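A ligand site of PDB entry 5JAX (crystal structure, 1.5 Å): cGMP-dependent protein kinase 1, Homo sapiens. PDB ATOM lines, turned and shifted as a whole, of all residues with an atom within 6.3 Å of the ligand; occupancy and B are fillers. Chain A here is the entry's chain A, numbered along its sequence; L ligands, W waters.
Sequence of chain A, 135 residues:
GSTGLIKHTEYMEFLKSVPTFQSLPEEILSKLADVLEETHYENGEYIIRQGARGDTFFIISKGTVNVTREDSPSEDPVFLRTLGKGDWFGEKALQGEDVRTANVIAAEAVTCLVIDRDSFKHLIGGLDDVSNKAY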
ATOM      1  N   ILE A  48      25.653  13.921  -9.550  1.00  0.00           N
ATOM      2  CA  ILE A  48      24.197  14.094  -9.495  1.00  0.00           C
ATOM      3  C   ILE A  48      23.813  14.217  -8.025  1.00  0.00           C
ATOM      4  O   ILE A  48      24.350  13.500  -7.174  1.00  0.00           O
ATOM      5  CB  ILE A  48      23.443  12.890 -10.110  1.00  0.00           C
ATOM      6  CG1 ILE A  48      23.660  12.833 -11.605  1.00  0.00           C
ATOM      7  CG2 ILE A  48      21.929  12.967  -9.776  1.00  0.00           C
ATOM      8  CD1 ILE A  48      23.085  11.587 -12.258  1.00  0.00           C
ATOM      9  N   THR A  56      20.168  14.746 -18.431  1.00  0.00           N
ATOM     10  CA  THR A  56      21.374  14.143 -18.993  1.00  0.00           C
ATOM     11  C   THR A  56      21.581  12.719 -18.508  1.00  0.00           C
ATOM     12  O   THR A  56      21.258  12.372 -17.363  1.00  0.00           O
ATOM     13  CB  THR A  56      22.619  14.967 -18.655  1.00  0.00           C
ATOM     14  OG1 THR A  56      22.581  15.354 -17.281  1.00  0.00           O
ATOM     15  CG2 THR A  56      22.717  16.203 -19.538  1.00  0.00           C
ATOM     16  N   VAL A  67      26.912   5.508  -5.382  1.00  0.00           N
ATOM     17  CA  VAL A  67      25.498   5.902  -5.473  1.00  0.00           C
ATOM     18  C   VAL A  67      24.875   5.797  -4.081  1.00  0.00           C
ATOM     19  O   VAL A  67      24.995   4.757  -3.419  1.00  0.00           O
ATOM     20  CB  VAL A  67      24.729   5.023  -6.464  1.00  0.00           C
ATOM     21  CG1 VAL A  67      23.302   5.534  -6.610  1.00  0.00           C
ATOM     22  CG2 VAL A  67      25.424   4.994  -7.798  1.00  0.00           C
ATOM     23  N   ARG A  69      21.273   7.183  -1.536  1.00  0.00           N
ATOM     24  CA  ARG A  69      19.897   7.673  -1.614  1.00  0.00           C
ATOM     25  C   ARG A  69      19.312   7.838  -0.220  1.00  0.00           C
ATOM     26  O   ARG A  69      19.525   6.984   0.651  1.00  0.00           O
ATOM     27  CB  ARG A  69      18.994   6.761  -2.447  1.00  0.00           C
ATOM     28  CG  ARG A  69      17.528   7.202  -2.486  1.00  0.00           C
ATOM     29  CD  ARG A  69      16.672   6.363  -3.412  1.00  0.00           C
ATOM     30  NE  ARG A  69      15.261   6.705  -3.283  1.00  0.00           N
ATOM     31  CZ  ARG A  69      14.694   7.784  -3.814  1.00  0.00           C
ATOM     32  N   LEU A  80      24.096   2.729  -1.857  1.00  0.00           N
ATOM     33  CA  LEU A  80      23.444   1.746  -2.705  1.00  0.00           C
ATOM     34  C   LEU A  80      24.446   0.843  -3.409  1.00  0.00           C
ATOM     35  O   LEU A  80      24.406  -0.388  -3.242  1.00  0.00           O
ATOM     36  CB  LEU A  80      22.507   2.417  -3.722  1.00  0.00           C
ATOM     37  CG  LEU A  80      21.406   3.283  -3.105  1.00  0.00           C
ATOM     38  CD1 LEU A  80      20.522   3.831  -4.204  1.00  0.00           C
ATOM     39  CD2 LEU A  80      20.580   2.512  -2.096  1.00  0.00           C
ATOM     40  N   ARG A  81      25.363   1.405  -4.200  1.00  0.00           N
ATOM     41  CA  ARG A  81      26.266   0.573  -4.981  1.00  0.00           C
ATOM     42  C   ARG A  81      27.393   1.433  -5.553  1.00  0.00           C
ATOM     43  O   ARG A  81      27.336   2.663  -5.531  1.00  0.00           O
ATOM     44  CB  ARG A  81      25.532  -0.115  -6.121  1.00  0.00           C
ATOM     45  CG  ARG A  81      25.225   0.816  -7.293  1.00  0.00           C
ATOM     46  CD  ARG A  81      24.256   0.186  -8.268  1.00  0.00           C
ATOM     47  NE  ARG A  81      22.902   0.140  -7.724  1.00  0.00           N
ATOM     48  CZ  ARG A  81      22.290  -0.946  -7.256  1.00  0.00           C
ATOM     49  NH1 ARG A  81      22.902  -2.130  -7.258  1.00  0.00           N
ATOM     50  NH2 ARG A  81      21.058  -0.841  -6.796  1.00  0.00           N
ATOM     51  N   LEU A  83      29.642   1.920  -9.169  1.00  0.00           N
ATOM     52  CA  LEU A  83      29.666   1.683 -10.596  1.00  0.00           C
ATOM     53  C   LEU A  83      31.048   2.034 -11.135  1.00  0.00           C
ATOM     54  O   LEU A  83      31.738   2.902 -10.586  1.00  0.00           O
ATOM     55  CB  LEU A  83      28.647   2.566 -11.328  1.00  0.00           C
ATOM     56  CG  LEU A  83      27.191   2.456 -10.958  1.00  0.00           C
ATOM     57  CD1 LEU A  83      26.477   3.536 -11.787  1.00  0.00           C
ATOM     58  CD2 LEU A  83      26.648   1.084 -11.241  1.00  0.00           C
ATOM     59  N   TRP A  88      26.597   2.861 -16.511  1.00  0.00           N
ATOM     60  CA  TRP A  88      25.870   4.063 -16.892  1.00  0.00           C
ATOM     61  C   TRP A  88      24.830   4.389 -15.821  1.00  0.00           C
ATOM     62  O   TRP A  88      24.441   3.529 -15.029  1.00  0.00           O
ATOM     63  CB  TRP A  88      25.237   3.945 -18.292  1.00  0.00           C
ATOM     64  CG  TRP A  88      24.518   2.650 -18.567  1.00  0.00           C
ATOM     65  CD1 TRP A  88      25.034   1.564 -19.223  1.00  0.00           C
ATOM     66  CD2 TRP A  88      23.173   2.314 -18.211  1.00  0.00           C
ATOM     67  NE1 TRP A  88      24.089   0.575 -19.288  1.00  0.00           N
ATOM     68  CE2 TRP A  88      22.941   1.001 -18.665  1.00  0.00           C
ATOM     69  CE3 TRP A  88      22.154   2.976 -17.538  1.00  0.00           C
ATOM     70  CZ2 TRP A  88      21.716   0.360 -18.482  1.00  0.00           C
ATOM     71  CZ3 TRP A  88      20.938   2.329 -17.345  1.00  0.00           C
ATOM     72  CH2 TRP A  88      20.742   1.027 -17.821  1.00  0.00           C
ATOM     73  N   PHE A  89      24.385   5.646 -15.804  1.00  0.00           N
ATOM     74  CA  PHE A  89      23.415   6.086 -14.806  1.00  0.00           C
ATOM     75  C   PHE A  89      22.787   7.393 -15.282  1.00  0.00           C
ATOM     76  O   PHE A  89      23.233   8.020 -16.241  1.00  0.00           O
ATOM     77  CB  PHE A  89      24.084   6.285 -13.434  1.00  0.00           C
ATOM     78  CG  PHE A  89      25.230   7.299 -13.442  1.00  0.00           C
ATOM     79  CD1 PHE A  89      24.974   8.637 -13.240  1.00  0.00           C
ATOM     80  CD2 PHE A  89      26.536   6.898 -13.657  1.00  0.00           C
ATOM     81  CE1 PHE A  89      25.989   9.563 -13.252  1.00  0.00           C
ATOM     82  CE2 PHE A  89      27.570   7.818 -13.667  1.00  0.00           C
ATOM     83  CZ  PHE A  89      27.294   9.159 -13.457  1.00  0.00           C
ATOM     84  N   GLY A  90      21.725   7.803 -14.595  1.00  0.00           N
ATOM     85  CA  GLY A  90      21.023   9.034 -14.928  1.00  0.00           C
ATOM     86  C   GLY A  90      19.815   8.852 -15.804  1.00  0.00           C
ATOM     87  O   GLY A  90      19.228   9.844 -16.253  1.00  0.00           O
ATOM     88  N   GLU A  91      19.381   7.615 -16.026  1.00  0.00           N
ATOM     89  CA  GLU A  91      18.264   7.384 -16.926  1.00  0.00           C
ATOM     90  C   GLU A  91      16.904   7.660 -16.291  1.00  0.00           C
ATOM     91  O   GLU A  91      15.943   7.922 -17.026  1.00  0.00           O
ATOM     92  CB  GLU A  91      18.305   5.946 -17.489  1.00  0.00           C
ATOM     93  CG  GLU A  91      17.710   4.836 -16.592  1.00  0.00           C
ATOM     94  CD  GLU A  91      18.570   4.476 -15.392  1.00  0.00           C
ATOM     95  OE1 GLU A  91      19.708   4.962 -15.269  1.00  0.00           O
ATOM     96  OE2 GLU A  91      18.129   3.662 -14.547  1.00  0.00           O
ATOM     97  N   LYS A  92      16.767   7.592 -14.972  1.00  0.00           N
ATOM     98  CA  LYS A  92      15.432   7.693 -14.390  1.00  0.00           C
ATOM     99  C   LYS A  92      14.821   9.075 -14.636  1.00  0.00           C
ATOM    100  O   LYS A  92      13.633   9.191 -14.947  1.00  0.00           O
ATOM    101  CB  LYS A  92      15.460   7.339 -12.901  1.00  0.00           C
ATOM    102  CG  LYS A  92      15.740   5.863 -12.652  1.00  0.00           C
ATOM    103  CD  LYS A  92      15.606   5.485 -11.191  1.00  0.00           C
ATOM    104  CE  LYS A  92      14.159   5.423 -10.758  1.00  0.00           C
ATOM    105  N   ALA A  93      15.627  10.133 -14.515  1.00  0.00           N
ATOM    106  CA  ALA A  93      15.121  11.472 -14.803  1.00  0.00           C
ATOM    107  C   ALA A  93      14.775  11.670 -16.279  1.00  0.00           C
ATOM    108  O   ALA A  93      14.129  12.664 -16.618  1.00  0.00           O
ATOM    109  CB  ALA A  93      16.137  12.529 -14.394  1.00  0.00           C
ATOM    110  N   LEU A  94      15.152  10.738 -17.151  1.00  0.00           N
ATOM    111  CA  LEU A  94      14.814  10.802 -18.557  1.00  0.00           C
ATOM    112  C   LEU A  94      13.648   9.888 -18.916  1.00  0.00           C
ATOM    113  O   LEU A  94      13.336   9.735 -20.098  1.00  0.00           O
ATOM    114  CB  LEU A  94      16.044  10.429 -19.406  1.00  0.00           C
ATOM    115  CG  LEU A  94      17.231  11.352 -19.181  1.00  0.00           C
ATOM    116  CD1 LEU A  94      18.488  10.806 -19.777  1.00  0.00           C
ATOM    117  CD2 LEU A  94      16.939  12.710 -19.772  1.00  0.00           C
ATOM    118  N   VAL A  99      12.966  14.196 -12.217  1.00  0.00           N
ATOM    119  CA  VAL A  99      13.643  14.331 -10.933  1.00  0.00           C
ATOM    120  C   VAL A  99      14.713  13.251 -10.758  1.00  0.00           C
ATOM    121  O   VAL A  99      14.519  12.086 -11.137  1.00  0.00           O
ATOM    122  CB  VAL A  99      12.623  14.315  -9.785  1.00  0.00           C
ATOM    123  CG1 VAL A  99      12.022  12.921  -9.597  1.00  0.00           C
ATOM    124  CG2 VAL A  99      13.263  14.821  -8.504  1.00  0.00           C
ATOM    125  N   ARG A 100      15.846  13.648 -10.171  1.00  0.00           N
ATOM    126  CA  ARG A 100      16.918  12.718  -9.828  1.00  0.00           C
ATOM    127  C   ARG A 100      16.556  11.985  -8.547  1.00  0.00           C
ATOM    128  O   ARG A 100      16.146  12.621  -7.568  1.00  0.00           O
ATOM    129  CB  ARG A 100      18.210  13.496  -9.619  1.00  0.00           C
ATOM    130  CG  ARG A 100      18.727  14.194 -10.865  1.00  0.00           C
ATOM    131  CD  ARG A 100      19.093  13.208 -11.966  1.00  0.00           C
ATOM    132  NE  ARG A 100      19.883  13.886 -12.996  1.00  0.00           N
ATOM    133  CZ  ARG A 100      20.166  13.376 -14.188  1.00  0.00           C
ATOM    134  NH1 ARG A 100      19.716  12.171 -14.498  1.00  0.00           N
ATOM    135  NH2 ARG A 100      20.875  14.065 -15.065  1.00  0.00           N
ATOM    136  N   THR A 101      16.713  10.675  -8.549  1.00  0.00           N
ATOM    137  CA  THR A 101      16.229   9.839  -7.471  1.00  0.00           C
ATOM    138  C   THR A 101      17.342   9.355  -6.555  1.00  0.00           C
ATOM    139  O   THR A 101      17.062   8.613  -5.611  1.00  0.00           O
ATOM    140  CB  THR A 101      15.465   8.644  -8.051  1.00  0.00           C
ATOM    141  OG1 THR A 101      16.339   7.821  -8.834  1.00  0.00           O
ATOM    142  CG2 THR A 101      14.343   9.110  -8.921  1.00  0.00           C
ATOM    143  N   ALA A 102      18.591   9.747  -6.798  1.00  0.00           N
ATOM    144  CA  ALA A 102      19.727   9.315  -5.989  1.00  0.00           C
ATOM    145  C   ALA A 102      20.896  10.244  -6.255  1.00  0.00           C
ATOM    146  O   ALA A 102      20.918  10.985  -7.247  1.00  0.00           O
ATOM    147  CB  ALA A 102      20.113   7.860  -6.312  1.00  0.00           C
ATOM    148  N   ASN A 103      21.851  10.215  -5.333  1.00  0.00           N
ATOM    149  CA  ASN A 103      23.123  10.914  -5.496  1.00  0.00           C
ATOM    150  C   ASN A 103      24.133  10.005  -6.190  1.00  0.00           C
ATOM    151  O   ASN A 103      24.169   8.799  -5.945  1.00  0.00           O
ATOM    152  CB  ASN A 103      23.714  11.308  -4.137  1.00  0.00           C
ATOM    153  CG  ASN A 103      22.773  12.127  -3.303  1.00  0.00           C
ATOM    154  OD1 ASN A 103      22.406  13.247  -3.662  1.00  0.00           O
ATOM    155  ND2 ASN A 103      22.368  11.570  -2.167  1.00  0.00           N
ATOM    156  N   VAL A 104      24.960  10.604  -7.037  1.00  0.00           N
ATOM    157  CA  VAL A 104      26.076   9.892  -7.657  1.00  0.00           C
ATOM    158  C   VAL A 104      27.312  10.736  -7.411  1.00  0.00           C
ATOM    159  O   VAL A 104      27.357  11.904  -7.797  1.00  0.00           O
ATOM    160  CB  VAL A 104      25.840   9.681  -9.164  1.00  0.00           C
ATOM    161  CG1 VAL A 104      26.989   8.878  -9.748  1.00  0.00           C
ATOM    162  CG2 VAL A 104      24.509   8.973  -9.406  1.00  0.00           C
ATOM    163  N   TYR A 135      16.118  -1.472  -9.976  1.00  0.00           N
ATOM    164  CA  TYR A 135      17.086  -1.597  -8.893  1.00  0.00           C
ATOM    165  C   TYR A 135      16.433  -2.228  -7.667  1.00  0.00           C
ATOM    166  O   TYR A 135      17.118  -2.721  -6.778  1.00  0.00           O
ATOM    167  CB  TYR A 135      17.653  -0.232  -8.532  1.00  0.00           C
ATOM    168  CG  TYR A 135      18.263   0.513  -9.709  1.00  0.00           C
ATOM    169  CD1 TYR A 135      19.593   0.341 -10.048  1.00  0.00           C
ATOM    170  CD2 TYR A 135      17.494   1.386 -10.466  1.00  0.00           C
ATOM    171  CE1 TYR A 135      20.145   1.022 -11.120  1.00  0.00           C
ATOM    172  CE2 TYR A 135      18.039   2.078 -11.535  1.00  0.00           C
ATOM    173  CZ  TYR A 135      19.362   1.886 -11.850  1.00  0.00           C
ATOM    174  OH  TYR A 135      19.922   2.560 -12.912  1.00  0.00           O
HETATM  175 BR1  LIG L   1      23.454   3.165 -10.355  1.00  0.00          BR
HETATM  176  C1  LIG L   1      21.780   3.400  -9.411  1.00  0.00           C
HETATM  177  N1  LIG L   1      21.407   2.515  -8.495  1.00  0.00           N
HETATM  178  C2  LIG L   1      20.237   3.027  -8.104  1.00  0.00           C
HETATM  179  C3  LIG L   1      19.215   2.610  -7.145  1.00  0.00           C
HETATM  180  O1  LIG L   1      19.399   1.575  -6.481  1.00  0.00           O
HETATM  181  N2  LIG L   1      18.137   3.377  -7.008  1.00  0.00           N
HETATM  182  C4  LIG L   1      17.953   4.506  -7.733  1.00  0.00           C
HETATM  183  N3  LIG L   1      16.830   5.207  -7.521  1.00  0.00           N
HETATM  184  N4  LIG L   1      18.835   4.954  -8.652  1.00  0.00           N
HETATM  185  C5  LIG L   1      19.974   4.271  -8.864  1.00  0.00           C
HETATM  186  N5  LIG L   1      20.996   4.441  -9.670  1.00  0.00           N
HETATM  187  C6  LIG L   1      21.247   5.537 -10.634  1.00  0.00           C
HETATM  188  C7  LIG L   1      20.117   5.696 -11.646  1.00  0.00           C
HETATM  189  O2  LIG L   1      20.713   5.693 -12.954  1.00  0.00           O
HETATM  190  O3  LIG L   1      21.415   6.764  -9.920  1.00  0.00           O
HETATM  191  C8  LIG L   1      20.822   7.744 -10.799  1.00  0.00           C
HETATM  192  C9  LIG L   1      20.531   9.094 -10.163  1.00  0.00           C
HETATM  193  O4  LIG L   1      19.886   9.870 -11.185  1.00  0.00           O
HETATM  194  C10 LIG L   1      19.571   7.075 -11.306  1.00  0.00           C
HETATM  195  O5  LIG L   1      18.935   7.803 -12.356  1.00  0.00           O
HETATM  196  P1  LIG L   1      18.563   9.303 -11.883  1.00  0.00           P
HETATM  197  O6  LIG L   1      17.512   9.196 -10.819  1.00  0.00           O
HETATM  198  O7  LIG L   1      18.282  10.134 -13.101  1.00  0.00           O
HETATM  199  O   HOH W   1      18.103  -0.194  -4.856  1.00  0.00           O
HETATM  200  O   HOH W   2      22.685   2.677 -12.935  1.00  0.00           O
HETATM  201  O   HOH W   3      15.918   3.012  -5.232  1.00  0.00           O
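O of Arg 81 sits at hydrogen-bond distance from N of Val 67 (2.9 Å).
O of Ile 48 sits at hydrogen-bond distance from N of Val 104 (3.0 Å).
The guanidinium group of Arg 100 lies within hydrogen-bond range of the backbone carbonyl oxygen of Thr 56 (2.9 Å).
N of Leu 80 is in hydrogen-bond range of O of Val 67, 2.7 Å away.
The backbone carbonyl oxygen (O) of Gly 90 sits at hydrogen-bond distance from the guanidinium group (NH1) of Arg 100.
OE2 of Glu 91 sits at hydrogen-bond distance from OH of Tyr 135, 2.7 Å away.
Water W1 lies within hydrogen-bond range of an oxygen (O1) of the ligand (2.7 Å) and the backbone carbonyl oxygen of Tyr 135 (3.3 Å).
Water W2 lies within hydrogen-bond range of the side-chain hydroxyl (OH) of Tyr 135 (2.8 Å) and the backbone carbonyl oxygen (O) of Trp 88 (2.9 Å).
The side-chain hydroxyl (OH) of Tyr 135 lies within hydrogen-bond range of an oxygen (O2) of the ligand (3.2 Å).
The backbone NH (N) of Ala 93 is in hydrogen-bond range of an oxygen (O7) of the ligand (3.0 Å).
An oxygen (O5) of the ligand is in hydrogen-bond range of the backbone NH (N) of Lys 92 (3.4 Å).
A nitrogen (N1) of the ligand is in hydrogen-bond range of the guanidinium group (NE) of Arg 81.
An oxygen (O2) of the ligand is in hydrogen-bond range of the backbone NH of Gly 90, 2.9 Å away.
The side-chain carboxylate (OE1) of Glu 91 sits at hydrogen-bond distance from an oxygen (O2) of the ligand.
The side-chain hydroxyl (OG1) of Thr 101 sits at hydrogen-bond distance from an oxygen (O6) of the ligand (2.7 Å).
The guanidinium group (NH1) of Arg 100 is in salt-bridge range of an oxygen (O7) of the ligand (2.9 Å).
O6 of the ligand lies within hydrogen-bond range of N of Thr 101 (2.8 Å).
CD1 of Ile 48 touches O4 of the ligand, 3.8 Å away.
Val 67 touches the ligand (CG2 to BR1, 3.7 Å).
CD1 of Leu 80 touches O1 of the ligand (3.4 Å).
CD1 of Leu 83 touches BR1 of the ligand (3.4 Å).
Phe 89 touches the ligand (CA to O2, 3.3 Å).
Ala 102 touches the ligand (O to C9, 3.5 Å).
CG2 of Val 104 touches O3 of the ligand (3.8 Å).
Hydrophobic or aromatic side chains within 4 Å of the ligand: Ile 48, Val 67, Leu 80, Leu 83, Phe 89, Ala 93, Ala 102, Val 104 and Tyr 135.
15 residues have an atom within 4 Å of the ligand: Ile 48, Val 67, Leu 80, Arg 81, Leu 83, Phe 89, Gly 90, Glu 91, Lys 92, Ala 93, Arg 100, Thr 101, Ala 102, Val 104 and Tyr 135.
Along chain A the residues within 4 Å of the ligand span positions 48 to 135.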
